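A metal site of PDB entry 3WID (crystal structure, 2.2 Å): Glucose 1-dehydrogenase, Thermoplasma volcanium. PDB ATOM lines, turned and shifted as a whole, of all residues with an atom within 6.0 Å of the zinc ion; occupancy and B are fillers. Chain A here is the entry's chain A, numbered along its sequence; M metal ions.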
ATOM      1  N   PRO A  96     -23.545  -0.795  12.530  1.00  0.00           N
ATOM      2  CA  PRO A  96     -22.707  -0.113  11.576  1.00  0.00           C
ATOM      3  C   PRO A  96     -22.235  -1.011  10.443  1.00  0.00           C
ATOM      4  O   PRO A  96     -21.957  -2.204  10.650  1.00  0.00           O
ATOM      5  CB  PRO A  96     -21.519   0.381  12.411  1.00  0.00           C
ATOM      6  CG  PRO A  96     -21.504  -0.460  13.615  1.00  0.00           C
ATOM      7  CD  PRO A  96     -22.922  -0.877  13.848  1.00  0.00           C
ATOM      8  N   GLY A  97     -22.178  -0.447   9.228  1.00  0.00           N
ATOM      9  CA  GLY A  97     -21.480  -1.056   8.111  1.00  0.00           C
ATOM     10  C   GLY A  97     -20.093  -0.505   8.106  1.00  0.00           C
ATOM     11  O   GLY A  97     -19.535  -0.335   9.143  1.00  0.00           O
ATOM     12  N   LYS A  98     -19.559  -0.198   6.927  1.00  0.00           N
ATOM     13  CA  LYS A  98     -18.193   0.266   6.821  1.00  0.00           C
ATOM     14  C   LYS A  98     -18.017   1.726   6.360  1.00  0.00           C
ATOM     15  O   LYS A  98     -16.921   2.217   6.436  1.00  0.00           O
ATOM     16  CB  LYS A  98     -17.446  -0.597   5.842  1.00  0.00           C
ATOM     17  CG  LYS A  98     -17.610  -2.076   6.070  1.00  0.00           C
ATOM     18  CD  LYS A  98     -16.824  -2.536   7.274  1.00  0.00           C
ATOM     19  CE  LYS A  98     -15.342  -2.712   6.938  1.00  0.00           C
ATOM     20  NZ  LYS A  98     -14.523  -3.036   8.143  1.00  0.00           N
ATOM     21  N   CYS A  99     -19.018   2.341   5.756  1.00  0.00           N
ATOM     22  CA  CYS A  99     -18.887   3.770   5.268  1.00  0.00           C
ATOM     23  C   CYS A  99     -18.351   4.785   6.282  1.00  0.00           C
ATOM     24  O   CYS A  99     -18.260   4.524   7.466  1.00  0.00           O
ATOM     25  CB  CYS A  99     -20.239   4.307   4.725  1.00  0.00           C
ATOM     26  SG  CYS A  99     -21.508   4.831   5.959  1.00  0.00           S
ATOM     27  N   VAL A 100     -18.081   5.984   5.800  1.00  0.00           N
ATOM     28  CA  VAL A 100     -17.484   7.061   6.571  1.00  0.00           C
ATOM     29  C   VAL A 100     -18.357   7.401   7.778  1.00  0.00           C
ATOM     30  O   VAL A 100     -17.851   7.720   8.831  1.00  0.00           O
ATOM     31  CB  VAL A 100     -17.136   8.262   5.643  1.00  0.00           C
ATOM     32  CG1 VAL A 100     -18.378   8.972   5.190  1.00  0.00           C
ATOM     33  CG2 VAL A 100     -16.181   9.242   6.334  1.00  0.00           C
ATOM     34  N   ASN A 101     -19.666   7.248   7.638  1.00  0.00           N
ATOM     35  CA  ASN A 101     -20.570   7.592   8.717  1.00  0.00           C
ATOM     36  C   ASN A 101     -20.762   6.465   9.722  1.00  0.00           C
ATOM     37  O   ASN A 101     -20.699   6.708  10.925  1.00  0.00           O
ATOM     38  CB  ASN A 101     -21.904   8.135   8.184  1.00  0.00           C
ATOM     39  CG  ASN A 101     -21.807   9.587   7.783  1.00  0.00           C
ATOM     40  OD1 ASN A 101     -21.847  10.448   8.645  1.00  0.00           O
ATOM     41  ND2 ASN A 101     -21.637   9.871   6.474  1.00  0.00           N
ATOM     42  N   CYS A 102     -20.883   5.236   9.261  1.00  0.00           N
ATOM     43  CA  CYS A 102     -20.971   4.067  10.099  1.00  0.00           C
ATOM     44  C   CYS A 102     -19.758   3.834  10.984  1.00  0.00           C
ATOM     45  O   CYS A 102     -19.899   3.379  12.082  1.00  0.00           O
ATOM     46  CB  CYS A 102     -21.220   2.834   9.256  1.00  0.00           C
ATOM     47  SG  CYS A 102     -22.922   2.504   8.861  1.00  0.00           S
ATOM     48  N   GLN A 107     -24.013   5.315  11.956  1.00  0.00           N
ATOM     49  CA  GLN A 107     -24.783   4.493  10.995  1.00  0.00           C
ATOM     50  C   GLN A 107     -26.207   4.990  10.750  1.00  0.00           C
ATOM     51  O   GLN A 107     -26.820   4.697   9.725  1.00  0.00           O
ATOM     52  CB  GLN A 107     -24.854   3.012  11.496  1.00  0.00           C
ATOM     53  CG  GLN A 107     -25.479   2.784  12.887  1.00  0.00           C
ATOM     54  CD  GLN A 107     -24.421   2.798  14.009  1.00  0.00           C
ATOM     55  OE1 GLN A 107     -23.521   3.641  14.023  1.00  0.00           O
ATOM     56  NE2 GLN A 107     -24.571   1.892  14.964  1.00  0.00           N
ATOM     57  N   ASN A 109     -26.757   7.669   9.904  1.00  0.00           N
ATOM     58  CA  ASN A 109     -26.524   8.513   8.724  1.00  0.00           C
ATOM     59  C   ASN A 109     -25.713   7.752   7.678  1.00  0.00           C
ATOM     60  O   ASN A 109     -24.900   8.351   7.017  1.00  0.00           O
ATOM     61  CB  ASN A 109     -25.803   9.821   9.103  1.00  0.00           C
ATOM     62  CG  ASN A 109     -26.678  10.747   9.936  1.00  0.00           C
ATOM     63  OD1 ASN A 109     -27.884  10.838   9.734  1.00  0.00           O
ATOM     64  ND2 ASN A 109     -26.048  11.537  10.776  1.00  0.00           N
ATOM     65  N   CYS A 110     -25.939   6.428   7.557  1.00  0.00           N
ATOM     66  CA  CYS A 110     -25.208   5.626   6.601  1.00  0.00           C
ATOM     67  C   CYS A 110     -25.210   6.245   5.194  1.00  0.00           C
ATOM     68  O   CYS A 110     -26.254   6.629   4.661  1.00  0.00           O
ATOM     69  CB  CYS A 110     -25.823   4.199   6.518  1.00  0.00           C
ATOM     70  SG  CYS A 110     -24.828   3.077   5.495  1.00  0.00           S
ATOM     71  N   SER A 111     -24.043   6.337   4.576  1.00  0.00           N
ATOM     72  CA  SER A 111     -23.944   6.907   3.213  1.00  0.00           C
ATOM     73  C   SER A 111     -24.328   5.934   2.089  1.00  0.00           C
ATOM     74  O   SER A 111     -24.534   6.386   0.974  1.00  0.00           O
ATOM     75  CB  SER A 111     -22.526   7.411   2.913  1.00  0.00           C
ATOM     76  OG  SER A 111     -22.052   8.297   3.890  1.00  0.00           O
ATOM     77  N   ILE A 112     -24.395   4.629   2.401  1.00  0.00           N
ATOM     78  CA  ILE A 112     -24.757   3.594   1.415  1.00  0.00           C
ATOM     79  C   ILE A 112     -26.182   3.155   1.596  1.00  0.00           C
ATOM     80  O   ILE A 112     -26.909   3.045   0.651  1.00  0.00           O
ATOM     81  CB  ILE A 112     -23.765   2.424   1.478  1.00  0.00           C
ATOM     82  CG1 ILE A 112     -22.357   2.940   1.151  1.00  0.00           C
ATOM     83  CG2 ILE A 112     -24.157   1.320   0.479  1.00  0.00           C
ATOM     84  CD1 ILE A 112     -21.296   1.894   1.299  1.00  0.00           C
ATOM     85  N   GLY A 113     -26.652   3.012   2.829  1.00  0.00           N
ATOM     86  CA  GLY A 113     -27.890   2.280   3.066  1.00  0.00           C
ATOM     87  C   GLY A 113     -27.657   0.783   3.097  1.00  0.00           C
ATOM     88  O   GLY A 113     -26.519   0.277   3.311  1.00  0.00           O
ATOM     89  N   ASP A 116     -24.818  -1.842   3.718  1.00  0.00           N
ATOM     90  CA  ASP A 116     -23.811  -1.389   4.658  1.00  0.00           C
ATOM     91  C   ASP A 116     -24.324  -1.463   6.115  1.00  0.00           C
ATOM     92  O   ASP A 116     -23.768  -2.190   6.930  1.00  0.00           O
ATOM     93  CB  ASP A 116     -23.325  -0.010   4.308  1.00  0.00           C
ATOM     94  CG  ASP A 116     -22.014   0.289   4.897  1.00  0.00           C
ATOM     95  OD1 ASP A 116     -21.162  -0.631   5.023  1.00  0.00           O
ATOM     96  OD2 ASP A 116     -21.800   1.446   5.305  1.00  0.00           O
ATOM     97  N   LYS A 117     -25.403  -0.779   6.429  1.00  0.00           N
ATOM     98  CA  LYS A 117     -26.017  -0.898   7.750  1.00  0.00           C
ATOM     99  C   LYS A 117     -27.081  -1.983   7.791  1.00  0.00           C
ATOM    100  O   LYS A 117     -27.623  -2.354   6.757  1.00  0.00           O
ATOM    101  CB  LYS A 117     -26.607   0.436   8.194  1.00  0.00           C
ATOM    102  CG  LYS A 117     -28.109   0.678   7.942  1.00  0.00           C
ATOM    103  CD  LYS A 117     -28.440   0.800   6.472  1.00  0.00           C
ATOM    104  CE  LYS A 117     -29.890   1.215   6.202  1.00  0.00           C
ATOM    105  NZ  LYS A 117     -30.932   0.424   6.868  1.00  0.00           N
HETATM  106 ZN    ZN M   1     -22.821   2.896   6.382  1.00  0.00          ZN
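The zinc ion is bound by the side-chain carboxylate (OD2) of Asp 116 (2.1 Å), the side-chain sulfur (SG) of Cys 110 (2.2 Å), the side-chain sulfur (SG) of Cys 99 (2.4 Å) and the side-chain sulfur (SG) of Cys 102 (2.5 Å).
The backbone NH of Gly 97 sits close to the backbone carbonyl oxygen of Asp 116 (3.3 Å).
The backbone NH of Lys 98 is in hydrogen-bond range of the side-chain carboxylate of Asp 116 (2.5 Å).
N of Ile 112 sits close to SG of Cys 110.
N of Gly 113 lies close to SG of Cys 110, at 3.2 Å.
The backbone NH of Ser 111 sits close to the side-chain sulfur of Cys 99 (3.3 Å).
The side-chain sulfur (SG) of Cys 99 sits close to the backbone NH (N) of Asn 101.
SG of Cys 102 sits close to N of Gly 97 (3.1 Å).
Within 4 Å of the zinc ion: Cys 99, Cys 102, Cys 110 and Asp 116.
The nearest printed residue that does not touch the zinc ion is Ser 111 (4.1 Å).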
